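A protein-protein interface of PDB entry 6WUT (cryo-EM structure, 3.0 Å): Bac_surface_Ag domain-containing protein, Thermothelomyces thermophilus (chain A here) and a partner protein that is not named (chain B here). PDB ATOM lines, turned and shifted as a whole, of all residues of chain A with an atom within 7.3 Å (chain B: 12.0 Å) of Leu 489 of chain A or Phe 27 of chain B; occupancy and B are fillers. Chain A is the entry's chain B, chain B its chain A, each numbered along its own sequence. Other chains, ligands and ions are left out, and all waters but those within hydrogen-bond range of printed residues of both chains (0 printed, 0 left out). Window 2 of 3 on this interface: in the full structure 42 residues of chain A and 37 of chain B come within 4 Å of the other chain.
The backbone NH (N) of Leu 29 of chain B sits at hydrogen-bond distance from the backbone carbonyl oxygen (O) of Leu 491 of chain A (2.7 Å). N of Arg 30 of chain B sits at hydrogen-bond distance from O of Leu 491 of chain A (3.5 Å).
The guanidinium group (NH2) of Arg 30 of chain B sits at hydrogen-bond distance from the side-chain hydroxyl (OH) of Tyr 32 of chain B. O of Leu 468 of chain A sits at hydrogen-bond distance from N of Leu 491 of chain A, at 3.1 Å. The backbone NH (N) of Leu 468 of chain A sits at hydrogen-bond distance from the backbone carbonyl oxygen (O) of Val 492 of chain A, at 3.1 Å. The backbone carbonyl oxygen of Ala 470 of chain A lies within hydrogen-bond range of the backbone NH of Leu 489 of chain A, at 3.1 Å.
Among the printed residues, merely in contact across the chains: Leu 489 of chain A with Phe 27 of chain B, Pro 490 of chain A with Phe 27 of chain B, Pro 490 of chain A with Pro 28 of chain B, Leu 491 of chain A with Phe 27 of chain B, Leu 491 of chain A with Pro 28 of chain B, Val 492 of chain A with Arg 30 of chain B and Lys 501 of chain A with Tyr 26 of chain B.
No residue of chain B comes within 4 Å of Gly 376 of chain A. Phe 377 of chain A touches none of the printed residues of chain B. No residue of chain B comes within 4 Å of Ala 470 of chain A. Val 472 of chain A touches none of the printed residues of chain B. Phe 487 of chain A touches none of the printed residues of chain B. Of chain B, only Phe 27 comes within 4 Å of Leu 489 of chain A. Pro 490 of chain A touches two residues of chain B. Leu 491 of chain A touches four residues of chain B. Lys 501 of chain A touches one residue of chain B. No residue of chain B comes within 4 Å of Gly 502 of chain A. Of the printed residues of chain A, Tyr 26 of chain B touches Lys 501. Of chain A, only Leu 489 (3.6 Å), Pro 490 (3.5 Å) and Leu 491 (3.6 Å) come within 4 Å of Phe 27 of chain B. Of the printed residues of chain A, Pro 28 of chain B touches Pro 490 (3.8 Å) and Leu 491 (3.5 Å). Printed residues of chain A within 4 Å of Leu 29 of chain B: Leu 491. Of the printed residues of chain A, Arg 30 of chain B touches Leu 491 and Val 492. The nearest residue of chain B that does not touch Leu 489 of chain A is Pro 28 of chain B (6.9 Å). The nearest residue of chain A that does not touch Phe 27 of chain B is Lys 501 of chain A (4.3 Å). The nearest printed residue of chain B that does not touch Val 492 of chain A is Tyr 32 of chain B (4.2 Å).
Of the 7 printed residues of chain B, 5 touch a printed residue of chain A. Printed residues of chain B that touch a printed residue of chain A: Tyr 26, Phe 27, Pro 28, Leu 29 and Arg 30. Hydrophobic or aromatic side chains of chain B within 4 Å of the printed part of chain A: Phe 27 and Leu 29. Among the printed residues, 9 pairs touch across the chains. Among the printed residues, no Asp or Glu carboxylate lies within 4 Å of a Lys or Arg side-chain nitrogen of the other chain.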
ATOM      1  N   ARG A 375      -3.709 -29.361 -32.815  1.00  0.00           N
ATOM      2  CA  ARG A 375      -5.023 -29.005 -33.327  1.00  0.00           C
ATOM      3  C   ARG A 375      -6.010 -28.757 -32.197  1.00  0.00           C
ATOM      4  O   ARG A 375      -6.108 -29.553 -31.263  1.00  0.00           O
ATOM      5  CB  ARG A 375      -5.536 -30.130 -34.219  1.00  0.00           C
ATOM      6  CG  ARG A 375      -5.427 -29.886 -35.697  1.00  0.00           C
ATOM      7  CD  ARG A 375      -4.336 -30.708 -36.346  1.00  0.00           C
ATOM      8  NE  ARG A 375      -4.327 -32.103 -35.935  1.00  0.00           N
ATOM      9  CZ  ARG A 375      -3.627 -33.045 -36.556  1.00  0.00           C
ATOM     10  NH1 ARG A 375      -2.898 -32.738 -37.618  1.00  0.00           N
ATOM     11  NH2 ARG A 375      -3.655 -34.294 -36.121  1.00  0.00           N
ATOM     12  N   GLY A 376      -6.739 -27.652 -32.287  1.00  0.00           N
ATOM     13  CA  GLY A 376      -7.754 -27.312 -31.311  1.00  0.00           C
ATOM     14  C   GLY A 376      -7.555 -25.984 -30.629  1.00  0.00           C
ATOM     15  O   GLY A 376      -8.365 -25.631 -29.763  1.00  0.00           O
ATOM     16  N   PHE A 377      -6.523 -25.223 -30.978  1.00  0.00           N
ATOM     17  CA  PHE A 377      -6.168 -24.002 -30.282  1.00  0.00           C
ATOM     18  C   PHE A 377      -5.909 -22.906 -31.303  1.00  0.00           C
ATOM     19  O   PHE A 377      -5.924 -23.138 -32.512  1.00  0.00           O
ATOM     20  CB  PHE A 377      -4.946 -24.218 -29.377  1.00  0.00           C
ATOM     21  CG  PHE A 377      -5.138 -25.310 -28.360  1.00  0.00           C
ATOM     22  CD1 PHE A 377      -5.832 -25.070 -27.193  1.00  0.00           C
ATOM     23  CD2 PHE A 377      -4.636 -26.572 -28.575  1.00  0.00           C
ATOM     24  CE1 PHE A 377      -6.027 -26.074 -26.268  1.00  0.00           C
ATOM     25  CE2 PHE A 377      -4.835 -27.573 -27.649  1.00  0.00           C
ATOM     26  CZ  PHE A 377      -5.524 -27.315 -26.496  1.00  0.00           C
ATOM     27  N   TYR A 421      -8.153 -37.382 -34.668  1.00  0.00           N
ATOM     28  CA  TYR A 421      -6.962 -37.036 -33.918  1.00  0.00           C
ATOM     29  C   TYR A 421      -7.280 -36.821 -32.445  1.00  0.00           C
ATOM     30  O   TYR A 421      -8.438 -36.726 -32.038  1.00  0.00           O
ATOM     31  CB  TYR A 421      -6.293 -35.793 -34.503  1.00  0.00           C
ATOM     32  CG  TYR A 421      -7.173 -34.578 -34.591  1.00  0.00           C
ATOM     33  CD1 TYR A 421      -7.279 -33.688 -33.530  1.00  0.00           C
ATOM     34  CD2 TYR A 421      -7.872 -34.299 -35.749  1.00  0.00           C
ATOM     35  CE1 TYR A 421      -8.077 -32.584 -33.611  1.00  0.00           C
ATOM     36  CE2 TYR A 421      -8.666 -33.192 -35.839  1.00  0.00           C
ATOM     37  CZ  TYR A 421      -8.764 -32.341 -34.767  1.00  0.00           C
ATOM     38  OH  TYR A 421      -9.558 -31.234 -34.866  1.00  0.00           O
ATOM     39  N   LEU A 468      -4.893 -30.611 -23.689  1.00  0.00           N
ATOM     40  CA  LEU A 468      -5.312 -31.617 -24.647  1.00  0.00           C
ATOM     41  C   LEU A 468      -6.566 -31.184 -25.394  1.00  0.00           C
ATOM     42  O   LEU A 468      -7.434 -30.508 -24.843  1.00  0.00           O
ATOM     43  CB  LEU A 468      -5.541 -32.941 -23.914  1.00  0.00           C
ATOM     44  CG  LEU A 468      -6.778 -33.793 -24.139  1.00  0.00           C
ATOM     45  CD1 LEU A 468      -6.464 -34.915 -25.101  1.00  0.00           C
ATOM     46  CD2 LEU A 468      -7.268 -34.343 -22.827  1.00  0.00           C
ATOM     47  N   ALA A 469      -6.641 -31.570 -26.667  1.00  0.00           N
ATOM     48  CA  ALA A 469      -7.824 -31.375 -27.493  1.00  0.00           C
ATOM     49  C   ALA A 469      -8.079 -32.648 -28.290  1.00  0.00           C
ATOM     50  O   ALA A 469      -7.323 -33.616 -28.207  1.00  0.00           O
ATOM     51  CB  ALA A 469      -7.672 -30.165 -28.414  1.00  0.00           C
ATOM     52  N   ALA A 470      -9.158 -32.645 -29.070  1.00  0.00           N
ATOM     53  CA  ALA A 470      -9.552 -33.797 -29.869  1.00  0.00           C
ATOM     54  C   ALA A 470     -10.339 -33.301 -31.072  1.00  0.00           C
ATOM     55  O   ALA A 470     -10.445 -32.097 -31.306  1.00  0.00           O
ATOM     56  CB  ALA A 470     -10.371 -34.786 -29.047  1.00  0.00           C
ATOM     57  N   GLY A 471     -10.873 -34.228 -31.854  1.00  0.00           N
ATOM     58  CA  GLY A 471     -11.720 -33.842 -32.963  1.00  0.00           C
ATOM     59  C   GLY A 471     -11.796 -34.907 -34.041  1.00  0.00           C
ATOM     60  O   GLY A 471     -11.332 -36.031 -33.872  1.00  0.00           O
ATOM     61  N   VAL A 472     -12.446 -34.522 -35.141  1.00  0.00           N
ATOM     62  CA  VAL A 472     -12.522 -35.284 -36.378  1.00  0.00           C
ATOM     63  C   VAL A 472     -12.040 -34.384 -37.511  1.00  0.00           C
ATOM     64  O   VAL A 472     -11.751 -33.208 -37.305  1.00  0.00           O
ATOM     65  CB  VAL A 472     -13.945 -35.805 -36.667  1.00  0.00           C
ATOM     66  CG1 VAL A 472     -14.479 -36.610 -35.509  1.00  0.00           C
ATOM     67  CG2 VAL A 472     -14.872 -34.656 -36.962  1.00  0.00           C
ATOM     68  N   PHE A 487     -12.845 -30.344 -37.272  1.00  0.00           N
ATOM     69  CA  PHE A 487     -13.795 -29.858 -36.272  1.00  0.00           C
ATOM     70  C   PHE A 487     -13.260 -30.281 -34.908  1.00  0.00           C
ATOM     71  O   PHE A 487     -13.353 -31.450 -34.532  1.00  0.00           O
ATOM     72  CB  PHE A 487     -15.185 -30.429 -36.542  1.00  0.00           C
ATOM     73  CG  PHE A 487     -16.140 -30.329 -35.377  1.00  0.00           C
ATOM     74  CD1 PHE A 487     -16.703 -29.116 -35.023  1.00  0.00           C
ATOM     75  CD2 PHE A 487     -16.508 -31.463 -34.666  1.00  0.00           C
ATOM     76  CE1 PHE A 487     -17.591 -29.034 -33.966  1.00  0.00           C
ATOM     77  CE2 PHE A 487     -17.394 -31.382 -33.608  1.00  0.00           C
ATOM     78  CZ  PHE A 487     -17.935 -30.168 -33.260  1.00  0.00           C
ATOM     79  N   SER A 488     -12.704 -29.330 -34.169  1.00  0.00           N
ATOM     80  CA  SER A 488     -11.988 -29.620 -32.938  1.00  0.00           C
ATOM     81  C   SER A 488     -12.817 -29.269 -31.712  1.00  0.00           C
ATOM     82  O   SER A 488     -13.825 -28.566 -31.794  1.00  0.00           O
ATOM     83  CB  SER A 488     -10.666 -28.859 -32.903  1.00  0.00           C
ATOM     84  OG  SER A 488     -10.843 -27.528 -33.349  1.00  0.00           O
ATOM     85  N   LEU A 489     -12.366 -29.758 -30.563  1.00  0.00           N
ATOM     86  CA  LEU A 489     -13.121 -29.653 -29.315  1.00  0.00           C
ATOM     87  C   LEU A 489     -12.143 -29.730 -28.156  1.00  0.00           C
ATOM     88  O   LEU A 489     -11.703 -30.827 -27.784  1.00  0.00           O
ATOM     89  CB  LEU A 489     -14.167 -30.759 -29.216  1.00  0.00           C
ATOM     90  CG  LEU A 489     -15.348 -30.566 -28.277  1.00  0.00           C
ATOM     91  CD1 LEU A 489     -16.088 -29.297 -28.626  1.00  0.00           C
ATOM     92  CD2 LEU A 489     -16.267 -31.761 -28.372  1.00  0.00           C
ATOM     93  N   PRO A 490     -11.770 -28.593 -27.564  1.00  0.00           N
ATOM     94  CA  PRO A 490     -10.782 -28.608 -26.477  1.00  0.00           C
ATOM     95  C   PRO A 490     -11.330 -29.243 -25.214  1.00  0.00           C
ATOM     96  O   PRO A 490     -12.500 -29.079 -24.869  1.00  0.00           O
ATOM     97  CB  PRO A 490     -10.473 -27.127 -26.263  1.00  0.00           C
ATOM     98  CG  PRO A 490     -10.839 -26.493 -27.496  1.00  0.00           C
ATOM     99  CD  PRO A 490     -12.039 -27.222 -27.999  1.00  0.00           C
ATOM    100  N   LEU A 491     -10.468 -29.967 -24.524  1.00  0.00           N
ATOM    101  CA  LEU A 491     -10.863 -30.731 -23.356  1.00  0.00           C
ATOM    102  C   LEU A 491     -10.220 -30.235 -22.076  1.00  0.00           C
ATOM    103  O   LEU A 491     -10.914 -30.050 -21.077  1.00  0.00           O
ATOM    104  CB  LEU A 491     -10.507 -32.204 -23.553  1.00  0.00           C
ATOM    105  CG  LEU A 491     -10.907 -32.840 -24.876  1.00  0.00           C
ATOM    106  CD1 LEU A 491     -10.476 -34.291 -24.905  1.00  0.00           C
ATOM    107  CD2 LEU A 491     -12.395 -32.737 -25.064  1.00  0.00           C
ATOM    108  N   VAL A 492      -8.904 -30.030 -22.077  1.00  0.00           N
ATOM    109  CA  VAL A 492      -8.163 -29.585 -20.907  1.00  0.00           C
ATOM    110  C   VAL A 492      -7.314 -28.394 -21.321  1.00  0.00           C
ATOM    111  O   VAL A 492      -6.604 -28.459 -22.327  1.00  0.00           O
ATOM    112  CB  VAL A 492      -7.300 -30.716 -20.322  1.00  0.00           C
ATOM    113  CG1 VAL A 492      -6.295 -30.183 -19.335  1.00  0.00           C
ATOM    114  CG2 VAL A 492      -8.183 -31.734 -19.640  1.00  0.00           C
ATOM    115  N   ARG A 500      -9.749 -22.923 -29.683  1.00  0.00           N
ATOM    116  CA  ARG A 500     -10.874 -22.788 -30.600  1.00  0.00           C
ATOM    117  C   ARG A 500     -11.729 -24.047 -30.585  1.00  0.00           C
ATOM    118  O   ARG A 500     -11.221 -25.156 -30.430  1.00  0.00           O
ATOM    119  CB  ARG A 500     -10.392 -22.512 -32.023  1.00  0.00           C
ATOM    120  CG  ARG A 500      -9.625 -21.222 -32.163  1.00  0.00           C
ATOM    121  CD  ARG A 500     -10.519 -20.023 -31.924  1.00  0.00           C
ATOM    122  NE  ARG A 500      -9.750 -18.807 -31.686  1.00  0.00           N
ATOM    123  CZ  ARG A 500      -9.610 -18.236 -30.495  1.00  0.00           C
ATOM    124  NH1 ARG A 500     -10.192 -18.762 -29.428  1.00  0.00           N
ATOM    125  NH2 ARG A 500      -8.892 -17.132 -30.371  1.00  0.00           N
ATOM    126  N   LYS A 501     -13.038 -23.874 -30.796  1.00  0.00           N
ATOM    127  CA  LYS A 501     -14.001 -24.918 -30.464  1.00  0.00           C
ATOM    128  C   LYS A 501     -14.820 -25.389 -31.662  1.00  0.00           C
ATOM    129  O   LYS A 501     -15.683 -26.258 -31.507  1.00  0.00           O
ATOM    130  CB  LYS A 501     -14.939 -24.421 -29.363  1.00  0.00           C
ATOM    131  CG  LYS A 501     -15.385 -25.466 -28.365  1.00  0.00           C
ATOM    132  CD  LYS A 501     -16.230 -24.834 -27.279  1.00  0.00           C
ATOM    133  CE  LYS A 501     -15.484 -23.713 -26.582  1.00  0.00           C
ATOM    134  NZ  LYS A 501     -16.350 -23.008 -25.608  1.00  0.00           N
ATOM    135  N   GLY A 502     -14.579 -24.856 -32.853  1.00  0.00           N
ATOM    136  CA  GLY A 502     -15.446 -25.193 -33.965  1.00  0.00           C
ATOM    137  C   GLY A 502     -14.737 -25.772 -35.166  1.00  0.00           C
ATOM    138  O   GLY A 502     -13.980 -26.733 -35.037  1.00  0.00           O
ATOM    139  N   TYR B  26     -18.292 -23.711 -22.400  1.00  0.00           N
ATOM    140  CA  TYR B  26     -18.884 -24.853 -21.716  1.00  0.00           C
ATOM    141  C   TYR B  26     -17.976 -26.078 -21.730  1.00  0.00           C
ATOM    142  O   TYR B  26     -17.833 -26.767 -20.722  1.00  0.00           O
ATOM    143  CB  TYR B  26     -20.233 -25.214 -22.346  1.00  0.00           C
ATOM    144  CG  TYR B  26     -20.700 -26.618 -22.026  1.00  0.00           C
ATOM    145  CD1 TYR B  26     -21.127 -26.952 -20.747  1.00  0.00           C
ATOM    146  CD2 TYR B  26     -20.725 -27.604 -23.004  1.00  0.00           C
ATOM    147  CE1 TYR B  26     -21.554 -28.231 -20.448  1.00  0.00           C
ATOM    148  CE2 TYR B  26     -21.150 -28.886 -22.714  1.00  0.00           C
ATOM    149  CZ  TYR B  26     -21.564 -29.193 -21.435  1.00  0.00           C
ATOM    150  OH  TYR B  26     -21.991 -30.466 -21.140  1.00  0.00           O
ATOM    151  N   PHE B  27     -17.393 -26.370 -22.880  1.00  0.00           N
ATOM    152  CA  PHE B  27     -16.705 -27.648 -22.990  1.00  0.00           C
ATOM    153  C   PHE B  27     -15.335 -27.839 -22.334  1.00  0.00           C
ATOM    154  O   PHE B  27     -15.065 -28.993 -21.976  1.00  0.00           O
ATOM    155  CB  PHE B  27     -16.577 -28.092 -24.446  1.00  0.00           C
ATOM    156  CG  PHE B  27     -16.764 -29.571 -24.607  1.00  0.00           C
ATOM    157  CD1 PHE B  27     -15.680 -30.421 -24.665  1.00  0.00           C
ATOM    158  CD2 PHE B  27     -18.036 -30.115 -24.623  1.00  0.00           C
ATOM    159  CE1 PHE B  27     -15.862 -31.777 -24.772  1.00  0.00           C
ATOM    160  CE2 PHE B  27     -18.222 -31.473 -24.736  1.00  0.00           C
ATOM    161  CZ  PHE B  27     -17.136 -32.304 -24.813  1.00  0.00           C
ATOM    162  N   PRO B  28     -14.429 -26.852 -22.188  1.00  0.00           N
ATOM    163  CA  PRO B  28     -13.120 -27.187 -21.592  1.00  0.00           C
ATOM    164  C   PRO B  28     -13.254 -27.645 -20.147  1.00  0.00           C
ATOM    165  O   PRO B  28     -13.500 -26.852 -19.238  1.00  0.00           O
ATOM    166  CB  PRO B  28     -12.335 -25.878 -21.697  1.00  0.00           C
ATOM    167  CG  PRO B  28     -12.843 -25.282 -22.910  1.00  0.00           C
ATOM    168  CD  PRO B  28     -14.316 -25.574 -22.921  1.00  0.00           C
ATOM    169  N   LEU B  29     -13.088 -28.959 -19.965  1.00  0.00           N
ATOM    170  CA  LEU B  29     -13.494 -29.688 -18.773  1.00  0.00           C
ATOM    171  C   LEU B  29     -12.564 -29.469 -17.597  1.00  0.00           C
ATOM    172  O   LEU B  29     -12.908 -29.856 -16.478  1.00  0.00           O
ATOM    173  CB  LEU B  29     -13.559 -31.188 -19.070  1.00  0.00           C
ATOM    174  CG  LEU B  29     -14.376 -31.714 -20.247  1.00  0.00           C
ATOM    175  CD1 LEU B  29     -14.041 -33.168 -20.512  1.00  0.00           C
ATOM    176  CD2 LEU B  29     -15.856 -31.554 -19.974  1.00  0.00           C
ATOM    177  N   ARG B  30     -11.395 -28.888 -17.822  1.00  0.00           N
ATOM    178  CA  ARG B  30     -10.424 -28.710 -16.759  1.00  0.00           C
ATOM    179  C   ARG B  30      -9.563 -27.518 -17.114  1.00  0.00           C
ATOM    180  O   ARG B  30      -8.872 -27.534 -18.134  1.00  0.00           O
ATOM    181  CB  ARG B  30      -9.558 -29.959 -16.580  1.00  0.00           C
ATOM    182  CG  ARG B  30      -9.682 -30.621 -15.230  1.00  0.00           C
ATOM    183  CD  ARG B  30      -8.944 -29.841 -14.167  1.00  0.00           C
ATOM    184  NE  ARG B  30      -9.091 -30.465 -12.858  1.00  0.00           N
ATOM    185  CZ  ARG B  30      -8.260 -31.379 -12.371  1.00  0.00           C
ATOM    186  NH1 ARG B  30      -8.471 -31.895 -11.168  1.00  0.00           N
ATOM    187  NH2 ARG B  30      -7.216 -31.775 -13.084  1.00  0.00           N
ATOM    188  N   ILE B  31      -9.626 -26.482 -16.291  1.00  0.00           N
ATOM    189  CA  ILE B  31      -8.831 -25.281 -16.479  1.00  0.00           C
ATOM    190  C   ILE B  31      -7.890 -25.172 -15.290  1.00  0.00           C
ATOM    191  O   ILE B  31      -8.326 -25.264 -14.138  1.00  0.00           O
ATOM    192  CB  ILE B  31      -9.719 -24.033 -16.613  1.00  0.00           C
ATOM    193  CG1 ILE B  31     -10.932 -24.347 -17.486  1.00  0.00           C
ATOM    194  CG2 ILE B  31      -8.957 -22.916 -17.261  1.00  0.00           C
ATOM    195  CD1 ILE B  31     -11.958 -23.267 -17.527  1.00  0.00           C
ATOM    196  N   TYR B  32      -6.603 -25.019 -15.569  1.00  0.00           N
ATOM    197  CA  TYR B  32      -5.598 -24.880 -14.532  1.00  0.00           C
ATOM    198  C   TYR B  32      -5.240 -23.412 -14.346  1.00  0.00           C
ATOM    199  O   TYR B  32      -5.671 -22.536 -15.096  1.00  0.00           O
ATOM    200  CB  TYR B  32      -4.343 -25.685 -14.878  1.00  0.00           C
ATOM    201  CG  TYR B  32      -4.446 -27.173 -14.672  1.00  0.00           C
ATOM    202  CD1 TYR B  32      -4.994 -27.995 -15.644  1.00  0.00           C
ATOM    203  CD2 TYR B  32      -3.969 -27.759 -13.513  1.00  0.00           C
ATOM    204  CE1 TYR B  32      -5.080 -29.356 -15.453  1.00  0.00           C
ATOM    205  CE2 TYR B  32      -4.052 -29.115 -13.318  1.00  0.00           C
ATOM    206  CZ  TYR B  32      -4.611 -29.905 -14.287  1.00  0.00           C
ATOM    207  OH  TYR B  32      -4.693 -31.259 -14.088  1.00  0.00           O
